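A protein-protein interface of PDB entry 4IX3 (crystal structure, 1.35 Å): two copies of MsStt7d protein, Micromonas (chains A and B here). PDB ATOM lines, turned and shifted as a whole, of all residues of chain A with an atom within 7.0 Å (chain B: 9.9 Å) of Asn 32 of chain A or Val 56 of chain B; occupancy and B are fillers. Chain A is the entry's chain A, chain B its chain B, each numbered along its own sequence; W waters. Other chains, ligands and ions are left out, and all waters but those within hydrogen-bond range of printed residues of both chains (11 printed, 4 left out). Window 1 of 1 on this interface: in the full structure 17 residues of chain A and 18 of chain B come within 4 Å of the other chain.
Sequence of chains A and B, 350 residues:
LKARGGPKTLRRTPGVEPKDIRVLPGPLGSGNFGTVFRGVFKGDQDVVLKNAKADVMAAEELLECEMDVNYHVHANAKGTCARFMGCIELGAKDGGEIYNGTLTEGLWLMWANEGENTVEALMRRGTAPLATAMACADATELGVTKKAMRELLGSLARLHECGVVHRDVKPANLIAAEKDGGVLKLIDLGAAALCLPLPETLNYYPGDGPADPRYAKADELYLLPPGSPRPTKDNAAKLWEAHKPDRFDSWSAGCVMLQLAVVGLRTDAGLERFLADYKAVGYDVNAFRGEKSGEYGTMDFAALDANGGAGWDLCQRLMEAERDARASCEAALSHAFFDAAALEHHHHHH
The backbone carbonyl oxygen of Ala 211 of chain A is in hydrogen-bond range of the backbone NH of Met 57 of chain B.
The guanidinium group of Arg 214 of chain A is in hydrogen-bond range of the backbone carbonyl oxygen of Ala 54 of chain B, 3.2 Å away.
The side-chain hydroxyl (OG) of Ser 30 of chain B sits close to the side-chain hydroxyl (OG) of Ser 30 of chain A, at 2.3 Å.
NZ of Lys 53 of chain B is in hydrogen-bond range of O of Ser 30 of chain A, at 3.2 Å.
The backbone carbonyl oxygen (O) of Gly 31 of chain B sits at hydrogen-bond distance from the side-chain amino group (NZ) of Lys 53 of chain A.
Val 56 of chain A touches Asn 32 of chain B (CG2 to OD1, 3.5 Å).
Met 57 of chain A touches Pro 210 of chain B.
Lys 170 of chain A touches Asp 55 of chain B.
OD2 of Asp 212 of chain A touches CB of Asp 55 of chain B, 3.2 Å away.
Pro 213 of chain A touches Asp 55 of chain B.
Val 56 of chain B touches Pro 213 of chain A.
Arg 214 of chain A touches Asp 55 of chain B.
No residue of chain B comes within 4 Å of Gly 34 of chain A.
Of the printed residues of chain B, Val 56 of chain A touches Asn 32.
Ala 59 of chain A touches none of the printed residues of chain B.
Printed residues of chain B within 4 Å of Lys 170 of chain A: Asp 55.
Val 56 of chain B touches just these residues of chain A: Asn 32 (3.5 Å) and Pro 213 (3.7 Å).
Ala 59 of chain B touches none of the printed residues of chain A.
Water W1 lies within hydrogen-bond range of OD2 of Asp 55 of chain B (2.7 Å), O of Ser 30 of chain A (2.9 Å) and NZ of Lys 53 of chain B (3.3 Å).
Water W10 lies within hydrogen-bond range of OD2 of Asp 55 of chain B (2.8 Å) and OD1 of Asn 32 of chain A (2.9 Å).
Water W4 lies within hydrogen-bond range of O of Asp 55 of chain B, NZ of Lys 170 of chain A and OD2 of Asp 168 of chain A.
Ser 30 of chain B touches its own counterpart, Ser 30 of chain A.
Asn 32 of chain A touches Val 56 of chain B, and with the chains exchanged Val 56 of chain A touches Asn 32 of chain B.
Of the 20 pairs that touch across the chains among the printed residues, 9 have their exchanged pair printed and touching as well.
Of the 21 printed residues of chain B, 10 touch a printed residue of chain A.
Printed residues of chain B that touch a printed residue of chain A: Ser 30, Gly 31, Asn 32, Lys 53, Ala 54, Asp 55, Val 56, Met 57, Pro 210 and Ala 211.
Hydrophobic or aromatic side chains of chain B that line the printed part of chain A: Ala 54, Val 56, Met 57 and Ala 211.
Of the 20 printed residues of chain A, 11 touch a printed residue of chain B.
Hydrophobic or aromatic side chains of chain A within 4 Å of the printed part of chain B: Val 56, Met 57, Ala 211 and Pro 213.
Among the printed residues, 20 pairs touch across the chains.
The side-chain carboxylate of Asp 168 of chain A lies within salt-bridge range of the side-chain amino group of Lys 170 of chain A, 2.8 Å away.
The backbone NH (N) of Lys 53 of chain A is in hydrogen-bond range of the backbone carbonyl oxygen (O) of Phe 33 of chain A, at 2.8 Å.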
ATOM      1  N   GLY A  29       4.998  23.133   1.142  1.00  0.00           N
ATOM      2  CA  GLY A  29       5.450  22.904  -0.223  1.00  0.00           C
ATOM      3  C   GLY A  29       6.780  22.185  -0.400  1.00  0.00           C
ATOM      4  O   GLY A  29       7.823  22.744  -0.061  1.00  0.00           O
ATOM      5  N   SER A  30       6.770  20.963  -0.944  1.00  0.00           N
ATOM      6  CA  SER A  30       8.015  20.350  -1.331  1.00  0.00           C
ATOM      7  C   SER A  30       8.614  21.128  -2.496  1.00  0.00           C
ATOM      8  O   SER A  30       7.898  21.666  -3.352  1.00  0.00           O
ATOM      9  CB  SER A  30       7.807  18.873  -1.665  1.00  0.00           C
ATOM     10  OG  SER A  30       6.508  18.667  -2.192  1.00  0.00           O
ATOM     11  N   GLY A  31       9.938  21.249  -2.458  1.00  0.00           N
ATOM     12  CA  GLY A  31      10.679  22.052  -3.413  1.00  0.00           C
ATOM     13  C   GLY A  31      11.363  21.001  -4.243  1.00  0.00           C
ATOM     14  O   GLY A  31      10.897  19.861  -4.321  1.00  0.00           O
ATOM     15  N   ASN A  32      12.555  21.306  -4.737  1.00  0.00           N
ATOM     16  CA  ASN A  32      13.175  20.385  -5.642  1.00  0.00           C
ATOM     17  C   ASN A  32      13.759  19.154  -4.956  1.00  0.00           C
ATOM     18  O   ASN A  32      13.745  18.087  -5.534  1.00  0.00           O
ATOM     19  CB  ASN A  32      14.256  21.059  -6.490  1.00  0.00           C
ATOM     20  CG  ASN A  32      13.677  22.155  -7.372  1.00  0.00           C
ATOM     21  OD1 ASN A  32      12.515  22.103  -7.759  1.00  0.00           O
ATOM     22  ND2 ASN A  32      14.468  23.190  -7.641  1.00  0.00           N
ATOM     23  N   PHE A  33      14.255  19.264  -3.720  1.00  0.00           N
ATOM     24  CA  PHE A  33      14.890  18.115  -3.074  1.00  0.00           C
ATOM     25  C   PHE A  33      14.463  17.870  -1.648  1.00  0.00           C
ATOM     26  O   PHE A  33      14.921  16.892  -1.060  1.00  0.00           O
ATOM     27  CB  PHE A  33      16.416  18.228  -3.156  1.00  0.00           C
ATOM     28  CG  PHE A  33      16.983  19.440  -2.455  1.00  0.00           C
ATOM     29  CD1 PHE A  33      17.159  19.431  -1.053  1.00  0.00           C
ATOM     30  CD2 PHE A  33      17.329  20.581  -3.184  1.00  0.00           C
ATOM     31  CE1 PHE A  33      17.660  20.565  -0.393  1.00  0.00           C
ATOM     32  CE2 PHE A  33      17.786  21.714  -2.527  1.00  0.00           C
ATOM     33  CZ  PHE A  33      17.963  21.694  -1.139  1.00  0.00           C
ATOM     34  N   GLY A  34      13.612  18.721  -1.090  1.00  0.00           N
ATOM     35  CA  GLY A  34      13.231  18.577   0.294  1.00  0.00           C
ATOM     36  C   GLY A  34      11.785  18.944   0.553  1.00  0.00           C
ATOM     37  O   GLY A  34      11.116  19.485  -0.348  1.00  0.00           O
ATOM     38  N   LYS A  50      12.750  21.210   7.722  1.00  0.00           N
ATOM     39  CA  LYS A  50      12.930  20.685   6.355  1.00  0.00           C
ATOM     40  C   LYS A  50      13.752  19.414   6.376  1.00  0.00           C
ATOM     41  O   LYS A  50      14.769  19.318   7.089  1.00  0.00           O
ATOM     42  CB  LYS A  50      13.636  21.699   5.464  1.00  0.00           C
ATOM     43  CG  LYS A  50      13.782  21.273   4.010  1.00  0.00           C
ATOM     44  CD  LYS A  50      14.410  22.347   3.159  1.00  0.00           C
ATOM     45  CE  LYS A  50      14.505  21.869   1.708  1.00  0.00           C
ATOM     46  NZ  LYS A  50      15.092  22.917   0.822  1.00  0.00           N
ATOM     47  N   LYS A  53      13.899  14.778   0.462  1.00  0.00           N
ATOM     48  CA  LYS A  53      12.993  13.833  -0.209  1.00  0.00           C
ATOM     49  C   LYS A  53      13.698  12.505  -0.438  1.00  0.00           C
ATOM     50  O   LYS A  53      14.779  12.476  -1.019  1.00  0.00           O
ATOM     51  CB  LYS A  53      12.563  14.461  -1.557  1.00  0.00           C
ATOM     52  CG  LYS A  53      11.532  15.597  -1.372  1.00  0.00           C
ATOM     53  CD  LYS A  53      11.146  16.251  -2.681  1.00  0.00           C
ATOM     54  CE  LYS A  53       9.764  15.823  -3.089  1.00  0.00           C
ATOM     55  NZ  LYS A  53       9.409  16.520  -4.359  1.00  0.00           N
ATOM     56  N   VAL A  56      14.437  11.669  -4.407  1.00  0.00           N
ATOM     57  CA  VAL A  56      15.226  12.575  -5.230  1.00  0.00           C
ATOM     58  C   VAL A  56      16.713  12.271  -5.104  1.00  0.00           C
ATOM     59  O   VAL A  56      17.240  12.199  -3.984  1.00  0.00           O
ATOM     60  CB  VAL A  56      14.889  14.062  -4.897  1.00  0.00           C
ATOM     61  CG1 VAL A  56      15.820  15.007  -5.628  1.00  0.00           C
ATOM     62  CG2 VAL A  56      13.433  14.373  -5.220  1.00  0.00           C
ATOM     63  N   MET A  57      17.382  12.158  -6.244  1.00  0.00           N
ATOM     64  CA  MET A  57      18.821  11.978  -6.337  1.00  0.00           C
ATOM     65  C   MET A  57      19.582  13.039  -5.546  1.00  0.00           C
ATOM     66  O   MET A  57      19.294  14.229  -5.696  1.00  0.00           O
ATOM     67  CB  MET A  57      19.181  12.100  -7.829  1.00  0.00           C
ATOM     68  CG  MET A  57      20.591  11.719  -8.229  1.00  0.00           C
ATOM     69  SD  MET A  57      20.704  11.670 -10.032  1.00  0.00           S
ATOM     70  CE  MET A  57      19.238  10.695 -10.280  1.00  0.00           C
ATOM     71  N   ALA A  59      19.485  14.122  -2.567  1.00  0.00           N
ATOM     72  CA  ALA A  59      18.726  15.073  -1.788  1.00  0.00           C
ATOM     73  C   ALA A  59      19.426  15.358  -0.469  1.00  0.00           C
ATOM     74  O   ALA A  59      19.439  16.482  -0.026  1.00  0.00           O
ATOM     75  CB  ALA A  59      17.315  14.572  -1.549  1.00  0.00           C
ATOM     76  N   LEU A  62      22.239  17.772  -1.051  1.00  0.00           N
ATOM     77  CA  LEU A  62      21.754  19.130  -1.359  1.00  0.00           C
ATOM     78  C   LEU A  62      21.330  19.787  -0.051  1.00  0.00           C
ATOM     79  O   LEU A  62      21.582  20.991   0.182  1.00  0.00           O
ATOM     80  CB  LEU A  62      20.577  19.033  -2.369  1.00  0.00           C
ATOM     81  CG  LEU A  62      21.037  18.648  -3.783  1.00  0.00           C
ATOM     82  CD1 LEU A  62      19.837  18.142  -4.595  1.00  0.00           C
ATOM     83  CD2 LEU A  62      21.789  19.806  -4.433  1.00  0.00           C
ATOM     84  N   ASP A 168      17.266  32.258  -5.647  1.00  0.00           N
ATOM     85  CA  ASP A 168      15.837  32.006  -5.763  1.00  0.00           C
ATOM     86  C   ASP A 168      15.032  33.153  -5.152  1.00  0.00           C
ATOM     87  O   ASP A 168      14.081  32.950  -4.395  1.00  0.00           O
ATOM     88  CB  ASP A 168      15.458  30.617  -5.192  1.00  0.00           C
ATOM     89  CG  ASP A 168      14.089  30.126  -5.704  1.00  0.00           C
ATOM     90  OD1 ASP A 168      13.571  29.156  -5.110  1.00  0.00           O
ATOM     91  OD2 ASP A 168      13.472  30.760  -6.580  1.00  0.00           O
ATOM     92  N   LYS A 170      12.256  35.798  -5.055  1.00  0.00           N
ATOM     93  CA  LYS A 170      10.928  35.964  -5.660  1.00  0.00           C
ATOM     94  C   LYS A 170       9.951  36.206  -4.530  1.00  0.00           C
ATOM     95  O   LYS A 170      10.230  35.927  -3.368  1.00  0.00           O
ATOM     96  CB  LYS A 170      10.488  34.701  -6.418  1.00  0.00           C
ATOM     97  CG  LYS A 170      10.526  33.391  -5.634  1.00  0.00           C
ATOM     98  CD  LYS A 170      10.068  32.206  -6.444  1.00  0.00           C
ATOM     99  CE  LYS A 170      10.137  30.876  -5.713  1.00  0.00           C
ATOM    100  NZ  LYS A 170      10.848  29.892  -6.559  1.00  0.00           N
ATOM    101  N   ALA A 191      19.151  26.654  -3.063  1.00  0.00           N
ATOM    102  CA  ALA A 191      19.980  26.746  -4.266  1.00  0.00           C
ATOM    103  C   ALA A 191      21.051  27.835  -4.142  1.00  0.00           C
ATOM    104  O   ALA A 191      21.721  28.140  -5.116  1.00  0.00           O
ATOM    105  CB  ALA A 191      19.134  27.018  -5.518  1.00  0.00           C
ATOM    106  N   PRO A 210      19.636  25.078 -11.063  1.00  0.00           N
ATOM    107  CA  PRO A 210      18.202  25.193 -10.802  1.00  0.00           C
ATOM    108  C   PRO A 210      17.884  26.669 -10.813  1.00  0.00           C
ATOM    109  O   PRO A 210      18.684  27.514 -10.395  1.00  0.00           O
ATOM    110  CB  PRO A 210      18.013  24.619  -9.411  1.00  0.00           C
ATOM    111  CG  PRO A 210      19.399  24.598  -8.814  1.00  0.00           C
ATOM    112  CD  PRO A 210      20.411  24.575  -9.916  1.00  0.00           C
ATOM    113  N   ALA A 211      16.760  26.996 -11.406  1.00  0.00           N
ATOM    114  CA  ALA A 211      16.307  28.380 -11.420  1.00  0.00           C
ATOM    115  C   ALA A 211      14.801  28.365 -11.515  1.00  0.00           C
ATOM    116  O   ALA A 211      14.225  27.485 -12.181  1.00  0.00           O
ATOM    117  CB  ALA A 211      16.836  29.082 -12.661  1.00  0.00           C
ATOM    118  N   ASP A 212      14.163  29.399 -10.991  1.00  0.00           N
ATOM    119  CA  ASP A 212      12.737  29.564 -11.216  1.00  0.00           C
ATOM    120  C   ASP A 212      12.593  30.337 -12.521  1.00  0.00           C
ATOM    121  O   ASP A 212      13.106  31.449 -12.633  1.00  0.00           O
ATOM    122  CB  ASP A 212      12.138  30.336 -10.049  1.00  0.00           C
ATOM    123  CG  ASP A 212      10.638  30.467 -10.170  1.00  0.00           C
ATOM    124  OD1 ASP A 212      10.113  30.721 -11.284  1.00  0.00           O
ATOM    125  OD2 ASP A 212       9.970  30.336  -9.162  1.00  0.00           O
ATOM    126  N   PRO A 213      11.988  29.762 -13.574  1.00  0.00           N
ATOM    127  CA  PRO A 213      12.009  30.429 -14.892  1.00  0.00           C
ATOM    128  C   PRO A 213      11.285  31.801 -14.864  1.00  0.00           C
ATOM    129  O   PRO A 213      11.614  32.655 -15.715  1.00  0.00           O
ATOM    130  CB  PRO A 213      11.256  29.421 -15.807  1.00  0.00           C
ATOM    131  CG  PRO A 213      10.394  28.639 -14.830  1.00  0.00           C
ATOM    132  CD  PRO A 213      11.207  28.508 -13.564  1.00  0.00           C
ATOM    133  N   ARG A 214      10.384  32.020 -13.917  1.00  0.00           N
ATOM    134  CA  ARG A 214       9.666  33.293 -13.862  1.00  0.00           C
ATOM    135  C   ARG A 214      10.622  34.431 -13.409  1.00  0.00           C
ATOM    136  O   ARG A 214      10.349  35.586 -13.730  1.00  0.00           O
ATOM    137  CB  ARG A 214       8.502  33.188 -12.909  1.00  0.00           C
ATOM    138  CG  ARG A 214       7.477  32.136 -13.297  1.00  0.00           C
ATOM    139  CD  ARG A 214       6.468  31.964 -12.222  1.00  0.00           C
ATOM    140  NE  ARG A 214       7.117  31.359 -11.040  1.00  0.00           N
ATOM    141  CZ  ARG A 214       6.562  31.263  -9.837  1.00  0.00           C
ATOM    142  NH1 ARG A 214       5.311  31.702  -9.593  1.00  0.00           N
ATOM    143  NH2 ARG A 214       7.283  30.691  -8.846  1.00  0.00           N
ATOM    144  N   SER B  30       3.431  16.597  -4.898  1.00  0.00           N
ATOM    145  CA  SER B  30       4.345  17.205  -5.857  1.00  0.00           C
ATOM    146  C   SER B  30       5.460  16.206  -6.206  1.00  0.00           C
ATOM    147  O   SER B  30       5.960  15.500  -5.332  1.00  0.00           O
ATOM    148  CB  SER B  30       4.949  18.457  -5.234  1.00  0.00           C
ATOM    149  OG  SER B  30       4.851  18.365  -3.827  1.00  0.00           O
ATOM    150  N   GLY B  31       5.811  16.109  -7.487  1.00  0.00           N
ATOM    151  CA  GLY B  31       6.884  15.226  -7.907  1.00  0.00           C
ATOM    152  C   GLY B  31       8.003  16.191  -8.184  1.00  0.00           C
ATOM    153  O   GLY B  31       8.126  17.196  -7.492  1.00  0.00           O
ATOM    154  N   ASN B  32       8.775  15.955  -9.234  1.00  0.00           N
ATOM    155  CA  ASN B  32       9.887  16.847  -9.494  1.00  0.00           C
ATOM    156  C   ASN B  32       9.448  18.112 -10.228  1.00  0.00           C
ATOM    157  O   ASN B  32      10.067  19.158 -10.018  1.00  0.00           O
ATOM    158  CB  ASN B  32      11.020  16.133 -10.250  1.00  0.00           C
ATOM    159  CG  ASN B  32      11.657  15.006  -9.427  1.00  0.00           C
ATOM    160  OD1 ASN B  32      11.717  15.077  -8.193  1.00  0.00           O
ATOM    161  ND2 ASN B  32      12.106  13.952 -10.097  1.00  0.00           N
ATOM    162  N   PHE B  33       8.516  18.010 -11.168  1.00  0.00           N
ATOM    163  CA  PHE B  33       8.212  19.155 -12.021  1.00  0.00           C
ATOM    164  C   PHE B  33       6.733  19.513 -12.067  1.00  0.00           C
ATOM    165  O   PHE B  33       6.413  20.513 -12.699  1.00  0.00           O
ATOM    166  CB  PHE B  33       8.769  18.984 -13.430  1.00  0.00           C
ATOM    167  CG  PHE B  33       8.118  17.836 -14.170  1.00  0.00           C
ATOM    168  CD1 PHE B  33       6.890  17.993 -14.802  1.00  0.00           C
ATOM    169  CD2 PHE B  33       8.733  16.583 -14.224  1.00  0.00           C
ATOM    170  CE1 PHE B  33       6.321  16.942 -15.517  1.00  0.00           C
ATOM    171  CE2 PHE B  33       8.163  15.533 -14.882  1.00  0.00           C
ATOM    172  CZ  PHE B  33       6.954  15.717 -15.546  1.00  0.00           C
ATOM    173  N   GLY B  34       5.882  18.705 -11.435  1.00  0.00           N
ATOM    174  CA  GLY B  34       4.432  18.928 -11.461  1.00  0.00           C
ATOM    175  C   GLY B  34       3.702  18.630 -10.168  1.00  0.00           C
ATOM    176  O   GLY B  34       4.294  18.130  -9.191  1.00  0.00           O
ATOM    177  N   THR B  35       2.418  18.936 -10.148  1.00  0.00           N
ATOM    178  CA  THR B  35       1.590  18.718  -8.981  1.00  0.00           C
ATOM    179  C   THR B  35       0.353  17.965  -9.408  1.00  0.00           C
ATOM    180  O   THR B  35      -0.280  18.326 -10.413  1.00  0.00           O
ATOM    181  CB  THR B  35       1.177  20.049  -8.315  1.00  0.00           C
ATOM    182  OG1 THR B  35       2.370  20.842  -8.122  1.00  0.00           O
ATOM    183  CG2 THR B  35       0.527  19.817  -6.968  1.00  0.00           C
ATOM    184  N   ASN B  51      -0.679  19.462 -13.201  1.00  0.00           N
ATOM    185  CA  ASN B  51      -0.155  20.617 -13.930  1.00  0.00           C
ATOM    186  C   ASN B  51       1.346  20.769 -13.626  1.00  0.00           C
ATOM    187  O   ASN B  51       1.906  19.975 -12.848  1.00  0.00           O
ATOM    188  CB  ASN B  51      -0.935  21.906 -13.627  1.00  0.00           C
ATOM    189  CG  ASN B  51      -0.675  22.448 -12.224  1.00  0.00           C
ATOM    190  OD1 ASN B  51      -0.124  21.746 -11.349  1.00  0.00           O
ATOM    191  ND2 ASN B  51      -1.089  23.708 -11.998  1.00  0.00           N
ATOM    192  N   ALA B  52       2.009  21.707 -14.292  1.00  0.00           N
ATOM    193  CA  ALA B  52       3.438  21.959 -14.069  1.00  0.00           C
ATOM    194  C   ALA B  52       3.610  22.797 -12.800  1.00  0.00           C
ATOM    195  O   ALA B  52       2.759  23.632 -12.457  1.00  0.00           O
ATOM    196  CB  ALA B  52       4.033  22.676 -15.279  1.00  0.00           C
ATOM    197  N   LYS B  53       4.736  22.617 -12.111  1.00  0.00           N
ATOM    198  CA  LYS B  53       5.157  23.555 -11.043  1.00  0.00           C
ATOM    199  C   LYS B  53       5.656  24.835 -11.695  1.00  0.00           C
ATOM    200  O   LYS B  53       6.514  24.775 -12.587  1.00  0.00           O
ATOM    201  CB  LYS B  53       6.275  22.906 -10.202  1.00  0.00           C
ATOM    202  CG  LYS B  53       5.685  21.813  -9.296  1.00  0.00           C
ATOM    203  CD  LYS B  53       6.784  21.124  -8.483  1.00  0.00           C
ATOM    204  CE  LYS B  53       7.258  21.959  -7.319  1.00  0.00           C
ATOM    205  NZ  LYS B  53       8.106  21.027  -6.525  1.00  0.00           N
ATOM    206  N   ALA B  54       5.139  25.972 -11.233  1.00  0.00           N
ATOM    207  CA  ALA B  54       5.546  27.249 -11.845  1.00  0.00           C
ATOM    208  C   ALA B  54       7.001  27.604 -11.558  1.00  0.00           C
ATOM    209  O   ALA B  54       7.616  28.449 -12.214  1.00  0.00           O
ATOM    210  CB  ALA B  54       4.672  28.351 -11.290  1.00  0.00           C
ATOM    211  N   ASP B  55       7.564  26.980 -10.520  1.00  0.00           N
ATOM    212  CA  ASP B  55       8.899  27.304 -10.004  1.00  0.00           C
ATOM    213  C   ASP B  55      10.032  26.427 -10.499  1.00  0.00           C
ATOM    214  O   ASP B  55      11.172  26.595 -10.038  1.00  0.00           O
ATOM    215  CB  ASP B  55       8.910  27.343  -8.482  1.00  0.00           C
ATOM    216  CG  ASP B  55       8.484  26.025  -7.859  1.00  0.00           C
ATOM    217  OD1 ASP B  55       7.563  25.343  -8.346  1.00  0.00           O
ATOM    218  OD2 ASP B  55       9.027  25.645  -6.797  1.00  0.00           O
ATOM    219  N   VAL B  56       9.763  25.524 -11.444  1.00  0.00           N
ATOM    220  CA  VAL B  56      10.756  24.566 -11.897  1.00  0.00           C
ATOM    221  C   VAL B  56      11.085  24.825 -13.364  1.00  0.00           C
ATOM    222  O   VAL B  56      10.210  24.886 -14.250  1.00  0.00           O
ATOM    223  CB  VAL B  56      10.231  23.128 -11.686  1.00  0.00           C
ATOM    224  CG1 VAL B  56      11.185  22.122 -12.354  1.00  0.00           C
ATOM    225  CG2 VAL B  56      10.031  22.858 -10.179  1.00  0.00           C
ATOM    226  N   MET B  57      12.370  24.963 -13.673  1.00  0.00           N
ATOM    227  CA  MET B  57      12.814  25.248 -15.022  1.00  0.00           C
ATOM    228  C   MET B  57      12.298  24.242 -16.051  1.00  0.00           C
ATOM    229  O   MET B  57      12.378  23.030 -15.835  1.00  0.00           O
ATOM    230  CB  MET B  57      14.347  25.265 -15.017  1.00  0.00           C
ATOM    231  CG  MET B  57      14.958  25.538 -16.372  1.00  0.00           C
ATOM    232  SD  MET B  57      14.345  27.086 -17.047  1.00  0.00           S
ATOM    233  CE  MET B  57      14.727  28.108 -15.645  1.00  0.00           C
ATOM    234  N   ALA B  58      11.699  24.713 -17.133  1.00  0.00           N
ATOM    235  CA  ALA B  58      11.307  23.660 -18.149  1.00  0.00           C
ATOM    236  C   ALA B  58      10.238  22.628 -17.711  1.00  0.00           C
ATOM    237  O   ALA B  58      10.053  21.603 -18.376  1.00  0.00           O
ATOM    238  CB  ALA B  58      12.521  22.871 -18.657  1.00  0.00           C
ATOM    239  N   ALA B  59       9.667  22.797 -16.523  1.00  0.00           N
ATOM    240  CA  ALA B  59       8.494  22.013 -16.142  1.00  0.00           C
ATOM    241  C   ALA B  59       7.439  21.979 -17.247  1.00  0.00           C
ATOM    242  O   ALA B  59       6.852  20.914 -17.474  1.00  0.00           O
ATOM    243  CB  ALA B  59       7.875  22.546 -14.870  1.00  0.00           C
ATOM    244  N   GLU B  60       7.193  23.060 -17.986  1.00  0.00           N
ATOM    245  CA  GLU B  60       6.211  22.929 -19.059  1.00  0.00           C
ATOM    246  C   GLU B  60       6.690  21.963 -20.123  1.00  0.00           C
ATOM    247  O   GLU B  60       5.913  21.177 -20.609  1.00  0.00           O
ATOM    248  CB  GLU B  60       5.647  24.238 -19.655  1.00  0.00           C
ATOM    249  CG  GLU B  60       6.317  24.821 -20.856  1.00  0.00           C
ATOM    250  CD  GLU B  60       5.853  26.256 -21.077  1.00  0.00           C
ATOM    251  OE1 GLU B  60       4.751  26.402 -21.658  1.00  0.00           O
ATOM    252  OE2 GLU B  60       6.502  27.212 -20.581  1.00  0.00           O
ATOM    253  N   GLU B  61       7.972  21.975 -20.445  1.00  0.00           N
ATOM    254  CA  GLU B  61       8.457  21.059 -21.484  1.00  0.00           C
ATOM    255  C   GLU B  61       8.398  19.621 -20.969  1.00  0.00           C
ATOM    256  O   GLU B  61       8.057  18.683 -21.708  1.00  0.00           O
ATOM    257  CB  GLU B  61       9.852  21.465 -21.944  1.00  0.00           C
ATOM    258  CG  GLU B  61       9.867  22.786 -22.733  1.00  0.00           C
ATOM    259  CD  GLU B  61       9.649  24.089 -21.925  1.00  0.00           C
ATOM    260  OE1 GLU B  61       9.851  24.175 -20.682  1.00  0.00           O
ATOM    261  OE2 GLU B  61       9.318  25.120 -22.562  1.00  0.00           O
ATOM    262  N   LEU B  62       8.691  19.413 -19.697  1.00  0.00           N
ATOM    263  CA  LEU B  62       8.610  18.051 -19.120  1.00  0.00           C
ATOM    264  C   LEU B  62       7.146  17.570 -19.080  1.00  0.00           C
ATOM    265  O   LEU B  62       6.876  16.398 -19.370  1.00  0.00           O
ATOM    266  CB  LEU B  62       9.227  18.050 -17.700  1.00  0.00           C
ATOM    267  CG  LEU B  62      10.746  18.227 -17.698  1.00  0.00           C
ATOM    268  CD1 LEU B  62      11.158  18.482 -16.261  1.00  0.00           C
ATOM    269  CD2 LEU B  62      11.440  16.994 -18.254  1.00  0.00           C
ATOM    270  N   LEU B  63       6.195  18.452 -18.751  1.00  0.00           N
ATOM    271  CA  LEU B  63       4.804  18.031 -18.757  1.00  0.00           C
ATOM    272  C   LEU B  63       4.357  17.740 -20.191  1.00  0.00           C
ATOM    273  O   LEU B  63       3.556  16.811 -20.409  1.00  0.00           O
ATOM    274  CB  LEU B  63       3.918  19.104 -18.120  1.00  0.00           C
ATOM    275  CG  LEU B  63       2.464  18.708 -17.865  1.00  0.00           C
ATOM    276  CD1 LEU B  63       2.378  17.671 -16.742  1.00  0.00           C
ATOM    277  CD2 LEU B  63       1.633  19.941 -17.470  1.00  0.00           C
ATOM    278  N   PRO B 210      16.635  11.990 -13.885  1.00  0.00           N
ATOM    279  CA  PRO B 210      16.065  11.948 -12.526  1.00  0.00           C
ATOM    280  C   PRO B 210      15.965  10.441 -12.278  1.00  0.00           C
ATOM    281  O   PRO B 210      15.947   9.636 -13.210  1.00  0.00           O
ATOM    282  CB  PRO B 210      14.689  12.620 -12.687  1.00  0.00           C
ATOM    283  CG  PRO B 210      14.341  12.290 -14.107  1.00  0.00           C
ATOM    284  CD  PRO B 210      15.604  12.212 -14.912  1.00  0.00           C
ATOM    285  N   ALA B 211      16.104  10.037 -11.040  1.00  0.00           N
ATOM    286  CA  ALA B 211      16.008   8.628 -10.751  1.00  0.00           C
ATOM    287  C   ALA B 211      15.674   8.695  -9.289  1.00  0.00           C
ATOM    288  O   ALA B 211      16.228   9.518  -8.543  1.00  0.00           O
ATOM    289  CB  ALA B 211      17.350   7.899 -10.994  1.00  0.00           C
HETATM  290  O   HOH W   1       7.704  23.957  -5.088  1.00  0.00           O
HETATM  291  O   HOH W   2      16.019  12.512  -8.894  1.00  0.00           O
HETATM  292  O   HOH W   3       9.992  27.529  -5.234  1.00  0.00           O
HETATM  293  O   HOH W   4      12.652  27.731  -7.742  1.00  0.00           O
HETATM  294  O   HOH W   5      14.687  24.189 -11.523  1.00  0.00           O
HETATM  295  O   HOH W   6       9.815  22.952  -6.635  1.00  0.00           O
HETATM  296  O   HOH W   7      12.766  19.562  -9.628  1.00  0.00           O
HETATM  297  O   HOH W   8      13.704  25.629  -9.233  1.00  0.00           O
HETATM  298  O   HOH W   9       7.716  13.682  -4.394  1.00  0.00           O
HETATM  299  O   HOH W  10      11.630  24.657  -6.786  1.00  0.00           O
HETATM  300  O   HOH W  11      13.953  17.569  -8.190  1.00  0.00           O
